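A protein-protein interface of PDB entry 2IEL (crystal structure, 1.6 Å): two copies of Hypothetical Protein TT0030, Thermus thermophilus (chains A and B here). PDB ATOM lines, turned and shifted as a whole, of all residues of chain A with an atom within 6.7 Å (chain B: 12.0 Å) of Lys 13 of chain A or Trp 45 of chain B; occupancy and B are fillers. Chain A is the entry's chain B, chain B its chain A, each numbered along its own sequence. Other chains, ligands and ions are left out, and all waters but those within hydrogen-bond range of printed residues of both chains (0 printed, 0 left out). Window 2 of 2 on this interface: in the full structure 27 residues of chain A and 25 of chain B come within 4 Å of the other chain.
N of Val 46 of chain B lies within hydrogen-bond range of OE1 of Glu 59 of chain A (3.4 Å).
The backbone carbonyl oxygen of His 9 of chain A is in hydrogen-bond range of the indole nitrogen of Trp 45 of chain B.
The side-chain carboxylate (OE2) of Glu 59 of chain A lies close to the backbone NH (N) of Trp 45 of chain B, 2.4 Å away.
His 9 of chain A touches Pro 43 of chain B (CE1 to O, 3.7 Å).
His 9 of chain A touches Gly 44 of chain B.
Arg 10 of chain A touches Pro 42 of chain B.
Arg 10 of chain A touches Pro 43 of chain B (CG to O, 3.2 Å).
Ala 12 of chain A touches Trp 45 of chain B.
Trp 45 of chain B touches Lys 13 of chain A (CH2 to CB, 3.2 Å).
Glu 58 of chain A touches Tyr 47 of chain B.
Glu 59 of chain A touches Gly 44 of chain B (OE2 to CA, 3.1 Å).
CB of Ala 62 of chain A touches CG2 of Val 46 of chain B, 3.8 Å away.
Trp 45 of chain B touches Ala 63 of chain A.
A ring nitrogen (NE2) of His 9 of chain A lies within hydrogen-bond range of the side-chain carboxylate (OE2) of Glu 59 of chain A, at 2.8 Å.
O of Ala 12 of chain A sits close to N of Leu 67 of chain A (3.5 Å).
O of Lys 13 of chain A sits close to OE1 of Gln 70 of chain A (3.0 Å).
The side-chain amide nitrogen of Gln 70 of chain A lies within hydrogen-bond range of the backbone carbonyl oxygen of Ala 12 of chain A (3.1 Å).
Hydrophobic or aromatic side chains of chain A within 4 Å of the printed part of chain B: His 9, Ala 12, Ala 62 and Ala 63.
Hydrophobic or aromatic side chains of chain B within 4 Å of the printed part of chain A: Pro 42, Pro 43, Trp 45, Val 46 and Tyr 47.
Among the printed residues, no Asp or Glu carboxylate lies within 4 Å of a Lys or Arg side-chain nitrogen of the other chain.
No position is printed for both chains.
Of the 16 pairs that touch across the chains among the printed residues, none has its exchanged pair printed and touching as well.
Of chain B, only Trp 45 (3.2 Å) comes within 4 Å of Lys 13 of chain A.
Printed residues of chain A within 4 Å of Trp 45 of chain B: His 9 (3.0 Å), Arg 10 (3.2 Å), Ala 12 (3.99 Å), Lys 13 (3.2 Å), Glu 59 (2.4 Å), Ala 62 (3.7 Å) and Ala 63 (3.6 Å).
His 9 of chain A touches three residues of chain B.
No residue of chain B comes within 4 Å of Thr 11 of chain A.
Of the printed residues of chain B, Glu 59 of chain A touches Gly 44, Trp 45 and Val 46.
Of the printed residues of chain B, Ala 63 of chain A touches Trp 45 (3.6 Å).
No residue of chain B comes within 4 Å of Ala 66 of chain A.
No residue of chain B comes within 4 Å of Leu 67 of chain A.
Of the printed residues of chain A, Pro 43 of chain B touches His 9 and Arg 10.
Of the printed residues of chain A, Val 46 of chain B touches Glu 58, Glu 59 and Ala 62.
Lys 64 of chain A touches none of the printed residues of chain B.
Val 37 of chain A touches none of the printed residues of chain B.
The nearest residue of chain B that does not touch Lys 13 of chain A is Gly 44 of chain B (10.0 Å).
The nearest printed residue of chain A that does not touch Trp 45 of chain B is Ala 66 of chain A (4.1 Å).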
ATOM      1  N   ALA A   8       6.447 -30.293  20.632  1.00  0.00           N
ATOM      2  CA  ALA A   8       5.159 -30.053  20.007  1.00  0.00           C
ATOM      3  C   ALA A   8       4.772 -28.596  20.147  1.00  0.00           C
ATOM      4  O   ALA A   8       5.150 -27.918  21.115  1.00  0.00           O
ATOM      5  CB  ALA A   8       4.073 -30.928  20.632  1.00  0.00           C
ATOM      6  N   HIS A   9       3.991 -28.134  19.184  1.00  0.00           N
ATOM      7  CA  HIS A   9       3.411 -26.817  19.242  1.00  0.00           C
ATOM      8  C   HIS A   9       1.964 -26.912  18.764  1.00  0.00           C
ATOM      9  O   HIS A   9       1.048 -27.004  19.575  1.00  0.00           O
ATOM     10  CB  HIS A   9       4.239 -25.831  18.421  1.00  0.00           C
ATOM     11  CG  HIS A   9       3.650 -24.458  18.366  1.00  0.00           C
ATOM     12  ND1 HIS A   9       3.690 -23.677  17.232  1.00  0.00           N
ATOM     13  CD2 HIS A   9       2.962 -23.748  19.291  1.00  0.00           C
ATOM     14  CE1 HIS A   9       3.079 -22.529  17.472  1.00  0.00           C
ATOM     15  NE2 HIS A   9       2.624 -22.552  18.710  1.00  0.00           N
ATOM     16  N   ARG A  10       1.767 -26.940  17.450  1.00  0.00           N
ATOM     17  CA  ARG A  10       0.425 -27.003  16.865  1.00  0.00           C
ATOM     18  C   ARG A  10      -0.317 -28.287  17.246  1.00  0.00           C
ATOM     19  O   ARG A  10      -1.534 -28.281  17.416  1.00  0.00           O
ATOM     20  CB  ARG A  10       0.511 -26.841  15.343  1.00  0.00           C
ATOM     21  CG  ARG A  10       1.086 -25.484  14.908  1.00  0.00           C
ATOM     22  CD  ARG A  10       1.865 -25.560  13.589  1.00  0.00           C
ATOM     23  NE  ARG A  10       0.997 -25.490  12.420  1.00  0.00           N
ATOM     24  CZ  ARG A  10       1.401 -25.547  11.150  1.00  0.00           C
ATOM     25  NH1 ARG A  10       2.695 -25.678  10.833  1.00  0.00           N
ATOM     26  NH2 ARG A  10       0.493 -25.474  10.184  1.00  0.00           N
ATOM     27  N   THR A  11       0.427 -29.376  17.412  1.00  0.00           N
ATOM     28  CA  THR A  11      -0.153 -30.687  17.697  1.00  0.00           C
ATOM     29  C   THR A  11      -0.352 -30.963  19.194  1.00  0.00           C
ATOM     30  O   THR A  11      -0.657 -32.097  19.574  1.00  0.00           O
ATOM     31  CB  THR A  11       0.706 -31.818  17.088  1.00  0.00           C
ATOM     32  OG1 THR A  11       2.019 -31.780  17.659  1.00  0.00           O
ATOM     33  CG2 THR A  11       0.795 -31.675  15.569  1.00  0.00           C
ATOM     34  N   ALA A  12      -0.160 -29.945  20.037  1.00  0.00           N
ATOM     35  CA  ALA A  12      -0.340 -30.096  21.492  1.00  0.00           C
ATOM     36  C   ALA A  12      -1.775 -30.481  21.895  1.00  0.00           C
ATOM     37  O   ALA A  12      -1.981 -31.060  22.965  1.00  0.00           O
ATOM     38  CB  ALA A  12       0.097 -28.847  22.224  1.00  0.00           C
ATOM     39  N   LYS A  13      -2.748 -30.156  21.043  1.00  0.00           N
ATOM     40  CA  LYS A  13      -4.166 -30.439  21.312  1.00  0.00           C
ATOM     41  C   LYS A  13      -4.633 -31.744  20.667  1.00  0.00           C
ATOM     42  O   LYS A  13      -5.761 -32.202  20.903  1.00  0.00           O
ATOM     43  CB  LYS A  13      -5.039 -29.274  20.837  1.00  0.00           C
ATOM     44  N   SER A  14      -3.757 -32.338  19.864  1.00  0.00           N
ATOM     45  CA  SER A  14      -4.087 -33.498  19.051  1.00  0.00           C
ATOM     46  C   SER A  14      -4.311 -34.767  19.876  1.00  0.00           C
ATOM     47  O   SER A  14      -3.551 -35.044  20.821  1.00  0.00           O
ATOM     48  CB  SER A  14      -2.976 -33.749  18.041  1.00  0.00           C
ATOM     49  OG  SER A  14      -1.837 -34.296  18.691  1.00  0.00           O
ATOM     50  N   PRO A  15      -5.331 -35.567  19.493  1.00  0.00           N
ATOM     51  CA  PRO A  15      -5.669 -36.769  20.254  1.00  0.00           C
ATOM     52  C   PRO A  15      -4.593 -37.833  20.135  1.00  0.00           C
ATOM     53  O   PRO A  15      -4.394 -38.609  21.074  1.00  0.00           O
ATOM     54  CB  PRO A  15      -6.967 -37.263  19.603  1.00  0.00           C
ATOM     55  CG  PRO A  15      -7.383 -36.213  18.620  1.00  0.00           C
ATOM     56  CD  PRO A  15      -6.184 -35.399  18.302  1.00  0.00           C
ATOM     57  N   GLU A  16      -3.911 -37.862  18.991  1.00  0.00           N
ATOM     58  CA  GLU A  16      -2.851 -38.830  18.725  1.00  0.00           C
ATOM     59  C   GLU A  16      -1.710 -38.711  19.734  1.00  0.00           C
ATOM     60  O   GLU A  16      -1.239 -39.718  20.257  1.00  0.00           O
ATOM     61  CB  GLU A  16      -2.315 -38.679  17.292  1.00  0.00           C
ATOM     62  CG  GLU A  16      -3.260 -39.167  16.185  1.00  0.00           C
ATOM     63  CD  GLU A  16      -4.167 -38.076  15.617  1.00  0.00           C
ATOM     64  OE1 GLU A  16      -4.182 -36.940  16.141  1.00  0.00           O
ATOM     65  OE2 GLU A  16      -4.870 -38.362  14.621  1.00  0.00           O
ATOM     66  N   LEU A  17      -1.276 -37.478  20.008  1.00  0.00           N
ATOM     67  CA  LEU A  17      -0.219 -37.233  20.994  1.00  0.00           C
ATOM     68  C   LEU A  17      -0.670 -37.615  22.404  1.00  0.00           C
ATOM     69  O   LEU A  17       0.069 -38.264  23.144  1.00  0.00           O
ATOM     70  CB  LEU A  17       0.249 -35.773  20.969  1.00  0.00           C
ATOM     71  CG  LEU A  17       1.259 -35.295  22.029  1.00  0.00           C
ATOM     72  CD1 LEU A  17       2.583 -36.050  21.959  1.00  0.00           C
ATOM     73  CD2 LEU A  17       1.490 -33.799  21.902  1.00  0.00           C
ATOM     74  N   ALA A  18      -1.876 -37.192  22.772  1.00  0.00           N
ATOM     75  CA  ALA A  18      -2.465 -37.609  24.034  1.00  0.00           C
ATOM     76  C   ALA A  18      -2.475 -39.134  24.120  1.00  0.00           C
ATOM     77  O   ALA A  18      -1.972 -39.702  25.083  1.00  0.00           O
ATOM     78  CB  ALA A  18      -3.867 -37.052  24.183  1.00  0.00           C
ATOM     79  N   VAL A  37       8.401 -26.151  23.185  1.00  0.00           N
ATOM     80  CA  VAL A  37       7.622 -25.555  22.111  1.00  0.00           C
ATOM     81  C   VAL A  37       8.520 -24.710  21.212  1.00  0.00           C
ATOM     82  O   VAL A  37       8.929 -23.609  21.563  1.00  0.00           O
ATOM     83  CB  VAL A  37       6.447 -24.708  22.678  1.00  0.00           C
ATOM     84  CG1 VAL A  37       5.677 -24.049  21.548  1.00  0.00           C
ATOM     85  CG2 VAL A  37       5.519 -25.570  23.539  1.00  0.00           C
ATOM     86  N   GLU A  58       4.129 -16.961  25.629  1.00  0.00           N
ATOM     87  CA  GLU A  58       2.664 -17.022  25.640  1.00  0.00           C
ATOM     88  C   GLU A  58       2.174 -18.184  24.789  1.00  0.00           C
ATOM     89  O   GLU A  58       1.263 -18.909  25.177  1.00  0.00           O
ATOM     90  CB  GLU A  58       2.044 -15.703  25.172  1.00  0.00           C
ATOM     91  CG  GLU A  58       2.367 -14.529  26.072  1.00  0.00           C
ATOM     92  CD  GLU A  58       1.427 -13.351  25.886  1.00  0.00           C
ATOM     93  OE1 GLU A  58       0.240 -13.566  25.530  1.00  0.00           O
ATOM     94  OE2 GLU A  58       1.888 -12.206  26.110  1.00  0.00           O
ATOM     95  N   GLU A  59       2.813 -18.378  23.634  1.00  0.00           N
ATOM     96  CA  GLU A  59       2.529 -19.517  22.769  1.00  0.00           C
ATOM     97  C   GLU A  59       2.765 -20.854  23.477  1.00  0.00           C
ATOM     98  O   GLU A  59       1.956 -21.776  23.360  1.00  0.00           O
ATOM     99  CB  GLU A  59       3.403 -19.429  21.519  1.00  0.00           C
ATOM    100  CG  GLU A  59       2.900 -20.231  20.355  1.00  0.00           C
ATOM    101  CD  GLU A  59       1.569 -19.741  19.802  1.00  0.00           C
ATOM    102  OE1 GLU A  59       1.352 -18.516  19.655  1.00  0.00           O
ATOM    103  OE2 GLU A  59       0.741 -20.613  19.495  1.00  0.00           O
ATOM    104  N   ALA A  60       3.875 -20.946  24.209  1.00  0.00           N
ATOM    105  CA  ALA A  60       4.222 -22.144  24.976  1.00  0.00           C
ATOM    106  C   ALA A  60       3.161 -22.450  26.049  1.00  0.00           C
ATOM    107  O   ALA A  60       2.700 -23.594  26.171  1.00  0.00           O
ATOM    108  CB  ALA A  60       5.603 -21.997  25.593  1.00  0.00           C
ATOM    109  N   ALA A  62       0.029 -21.554  26.019  1.00  0.00           N
ATOM    110  CA  ALA A  62      -1.204 -21.961  25.346  1.00  0.00           C
ATOM    111  C   ALA A  62      -1.156 -23.425  24.908  1.00  0.00           C
ATOM    112  O   ALA A  62      -2.148 -24.159  25.006  1.00  0.00           O
ATOM    113  CB  ALA A  62      -1.479 -21.057  24.152  1.00  0.00           C
ATOM    114  N   ALA A  63       0.008 -23.853  24.422  1.00  0.00           N
ATOM    115  CA  ALA A  63       0.201 -25.243  24.039  1.00  0.00           C
ATOM    116  C   ALA A  63       0.129 -26.162  25.264  1.00  0.00           C
ATOM    117  O   ALA A  63      -0.466 -27.236  25.201  1.00  0.00           O
ATOM    118  CB  ALA A  63       1.532 -25.408  23.296  1.00  0.00           C
ATOM    119  N   LYS A  64       0.701 -25.712  26.379  1.00  0.00           N
ATOM    120  CA  LYS A  64       0.645 -26.472  27.630  1.00  0.00           C
ATOM    121  C   LYS A  64      -0.800 -26.663  28.106  1.00  0.00           C
ATOM    122  O   LYS A  64      -1.172 -27.760  28.504  1.00  0.00           O
ATOM    123  CB  LYS A  64       1.503 -25.822  28.710  1.00  0.00           C
ATOM    124  CG  LYS A  64       1.509 -26.564  30.044  1.00  0.00           C
ATOM    125  CD  LYS A  64       2.378 -25.814  31.026  1.00  0.00           C
ATOM    126  CE  LYS A  64       2.499 -26.520  32.356  1.00  0.00           C
ATOM    127  NZ  LYS A  64       2.901 -25.494  33.347  1.00  0.00           N
ATOM    128  N   ALA A  66      -3.486 -26.736  26.256  1.00  0.00           N
ATOM    129  CA  ALA A  66      -4.101 -27.658  25.300  1.00  0.00           C
ATOM    130  C   ALA A  66      -3.793 -29.121  25.611  1.00  0.00           C
ATOM    131  O   ALA A  66      -4.669 -29.987  25.520  1.00  0.00           O
ATOM    132  CB  ALA A  66      -3.659 -27.316  23.867  1.00  0.00           C
ATOM    133  N   LEU A  67      -2.537 -29.388  25.953  1.00  0.00           N
ATOM    134  CA  LEU A  67      -2.082 -30.729  26.309  1.00  0.00           C
ATOM    135  C   LEU A  67      -2.682 -31.194  27.645  1.00  0.00           C
ATOM    136  O   LEU A  67      -3.166 -32.321  27.757  1.00  0.00           O
ATOM    137  CB  LEU A  67      -0.552 -30.768  26.348  1.00  0.00           C
ATOM    138  CG  LEU A  67       0.179 -32.105  26.498  1.00  0.00           C
ATOM    139  CD1 LEU A  67      -0.376 -33.193  25.584  1.00  0.00           C
ATOM    140  CD2 LEU A  67       1.658 -31.904  26.250  1.00  0.00           C
ATOM    141  N   GLN A  70      -6.241 -32.363  27.544  1.00  0.00           N
ATOM    142  CA  GLN A  70      -6.424 -33.723  27.039  1.00  0.00           C
ATOM    143  C   GLN A  70      -6.272 -34.783  28.132  1.00  0.00           C
ATOM    144  O   GLN A  70      -6.574 -35.956  27.906  1.00  0.00           O
ATOM    145  CB  GLN A  70      -5.436 -34.009  25.910  1.00  0.00           C
ATOM    146  CG  GLN A  70      -5.607 -33.124  24.701  1.00  0.00           C
ATOM    147  CD  GLN A  70      -5.092 -33.788  23.451  1.00  0.00           C
ATOM    148  OE1 GLN A  70      -5.803 -34.571  22.813  1.00  0.00           O
ATOM    149  NE2 GLN A  70      -3.843 -33.484  23.090  1.00  0.00           N
ATOM    150  N   PRO B  41       6.798 -17.262  10.865  1.00  0.00           N
ATOM    151  CA  PRO B  41       6.603 -18.465  11.665  1.00  0.00           C
ATOM    152  C   PRO B  41       5.289 -19.189  11.316  1.00  0.00           C
ATOM    153  O   PRO B  41       4.364 -18.564  10.784  1.00  0.00           O
ATOM    154  CB  PRO B  41       6.526 -17.922  13.093  1.00  0.00           C
ATOM    155  CG  PRO B  41       6.013 -16.565  12.952  1.00  0.00           C
ATOM    156  CD  PRO B  41       6.525 -16.036  11.640  1.00  0.00           C
ATOM    157  N   PRO B  42       5.186 -20.491  11.645  1.00  0.00           N
ATOM    158  CA  PRO B  42       3.939 -21.188  11.353  1.00  0.00           C
ATOM    159  C   PRO B  42       2.786 -20.705  12.250  1.00  0.00           C
ATOM    160  O   PRO B  42       3.034 -19.985  13.236  1.00  0.00           O
ATOM    161  CB  PRO B  42       4.277 -22.664  11.627  1.00  0.00           C
ATOM    162  CG  PRO B  42       5.449 -22.646  12.522  1.00  0.00           C
ATOM    163  CD  PRO B  42       6.189 -21.373  12.282  1.00  0.00           C
ATOM    164  N   PRO B  43       1.540 -21.085  11.904  1.00  0.00           N
ATOM    165  CA  PRO B  43       0.359 -20.752  12.721  1.00  0.00           C
ATOM    166  C   PRO B  43       0.505 -21.259  14.152  1.00  0.00           C
ATOM    167  O   PRO B  43       1.101 -22.313  14.379  1.00  0.00           O
ATOM    168  CB  PRO B  43      -0.783 -21.492  12.011  1.00  0.00           C
ATOM    169  CG  PRO B  43      -0.321 -21.678  10.616  1.00  0.00           C
ATOM    170  CD  PRO B  43       1.169 -21.875  10.716  1.00  0.00           C
ATOM    171  N   GLY B  44      -0.012 -20.486  15.105  1.00  0.00           N
ATOM    172  CA  GLY B  44      -0.004 -20.878  16.516  1.00  0.00           C
ATOM    173  C   GLY B  44      -1.371 -20.758  17.166  1.00  0.00           C
ATOM    174  O   GLY B  44      -2.392 -20.629  16.476  1.00  0.00           O
ATOM    175  N   TRP B  45      -1.380 -20.801  18.497  1.00  0.00           N
ATOM    176  CA  TRP B  45      -2.610 -20.759  19.295  1.00  0.00           C
ATOM    177  C   TRP B  45      -3.045 -19.339  19.625  1.00  0.00           C
ATOM    178  O   TRP B  45      -4.236 -19.085  19.837  1.00  0.00           O
ATOM    179  CB  TRP B  45      -2.412 -21.495  20.624  1.00  0.00           C
ATOM    180  CG  TRP B  45      -1.903 -22.883  20.508  1.00  0.00           C
ATOM    181  CD1 TRP B  45      -0.605 -23.292  20.617  1.00  0.00           C
ATOM    182  CD2 TRP B  45      -2.675 -24.058  20.259  1.00  0.00           C
ATOM    183  NE1 TRP B  45      -0.523 -24.651  20.454  1.00  0.00           N
ATOM    184  CE2 TRP B  45      -1.778 -25.147  20.231  1.00  0.00           C
ATOM    185  CE3 TRP B  45      -4.042 -24.299  20.051  1.00  0.00           C
ATOM    186  CZ2 TRP B  45      -2.199 -26.458  20.009  1.00  0.00           C
ATOM    187  CZ3 TRP B  45      -4.463 -25.606  19.829  1.00  0.00           C
ATOM    188  CH2 TRP B  45      -3.540 -26.666  19.810  1.00  0.00           C
ATOM    189  N   VAL B  46      -2.081 -18.423  19.693  1.00  0.00           N
ATOM    190  CA  VAL B  46      -2.325 -17.086  20.228  1.00  0.00           C
ATOM    191  C   VAL B  46      -2.456 -16.054  19.110  1.00  0.00           C
ATOM    192  O   VAL B  46      -3.503 -15.414  18.982  1.00  0.00           O
ATOM    193  CB  VAL B  46      -1.236 -16.666  21.263  1.00  0.00           C
ATOM    194  CG1 VAL B  46      -1.558 -15.319  21.880  1.00  0.00           C
ATOM    195  CG2 VAL B  46      -1.108 -17.716  22.351  1.00  0.00           C
ATOM    196  N   TYR B  47      -1.400 -15.915  18.303  1.00  0.00           N
ATOM    197  CA  TYR B  47      -1.360 -14.950  17.205  1.00  0.00           C
ATOM    198  C   TYR B  47      -1.399 -15.657  15.858  1.00  0.00           C
ATOM    199  O   TYR B  47      -2.392 -15.579  15.137  1.00  0.00           O
ATOM    200  CB  TYR B  47      -0.105 -14.077  17.297  1.00  0.00           C
ATOM    201  CG  TYR B  47       0.071 -13.389  18.631  1.00  0.00           C
ATOM    202  CD1 TYR B  47      -0.630 -12.221  18.932  1.00  0.00           C
ATOM    203  CD2 TYR B  47       0.934 -13.911  19.597  1.00  0.00           C
ATOM    204  CE1 TYR B  47      -0.473 -11.586  20.162  1.00  0.00           C
ATOM    205  CE2 TYR B  47       1.101 -13.282  20.829  1.00  0.00           C
ATOM    206  CZ  TYR B  47       0.391 -12.123  21.102  1.00  0.00           C
ATOM    207  OH  TYR B  47       0.550 -11.498  22.318  1.00  0.00           O
ATOM    208  N   ASN B  50      -2.734 -13.319   9.789  1.00  0.00           N
ATOM    209  CA  ASN B  50      -2.647 -11.995   9.180  1.00  0.00           C
ATOM    210  C   ASN B  50      -1.715 -11.056   9.932  1.00  0.00           C
ATOM    211  O   ASN B  50      -0.943 -10.323   9.312  1.00  0.00           O
ATOM    212  CB  ASN B  50      -4.037 -11.354   9.057  1.00  0.00           C
ATOM    213  CG  ASN B  50      -4.963 -12.124   8.132  1.00  0.00           C
ATOM    214  OD1 ASN B  50      -4.573 -12.539   7.039  1.00  0.00           O
ATOM    215  ND2 ASN B  50      -6.209 -12.308   8.566  1.00  0.00           N
ATOM    216  N   GLU B  51      -1.800 -11.066  11.265  1.00  0.00           N
ATOM    217  CA  GLU B  51      -0.926 -10.236  12.097  1.00  0.00           C
ATOM    218  C   GLU B  51       0.519 -10.741  12.024  1.00  0.00           C
ATOM    219  O   GLU B  51       1.457  -9.947  11.906  1.00  0.00           O
ATOM    220  CB  GLU B  51      -1.446 -10.172  13.545  1.00  0.00           C
ATOM    221  CG  GLU B  51      -0.439  -9.697  14.614  1.00  0.00           C
ATOM    222  CD  GLU B  51      -0.028  -8.220  14.502  1.00  0.00           C
ATOM    223  OE1 GLU B  51      -0.352  -7.558  13.488  1.00  0.00           O
ATOM    224  OE2 GLU B  51       0.644  -7.720  15.439  1.00  0.00           O
ATOM    225  N   VAL B  52       0.681 -12.061  12.078  1.00  0.00           N
ATOM    226  CA  VAL B  52       2.001 -12.698  11.987  1.00  0.00           C
ATOM    227  C   VAL B  52       2.651 -12.383  10.633  1.00  0.00           C
ATOM    228  O   VAL B  52       3.835 -12.032  10.570  1.00  0.00           O
ATOM    229  CB  VAL B  52       1.910 -14.232  12.246  1.00  0.00           C
ATOM    230  CG1 VAL B  52       3.130 -14.966  11.734  1.00  0.00           C
ATOM    231  CG2 VAL B  52       1.713 -14.517  13.731  1.00  0.00           C
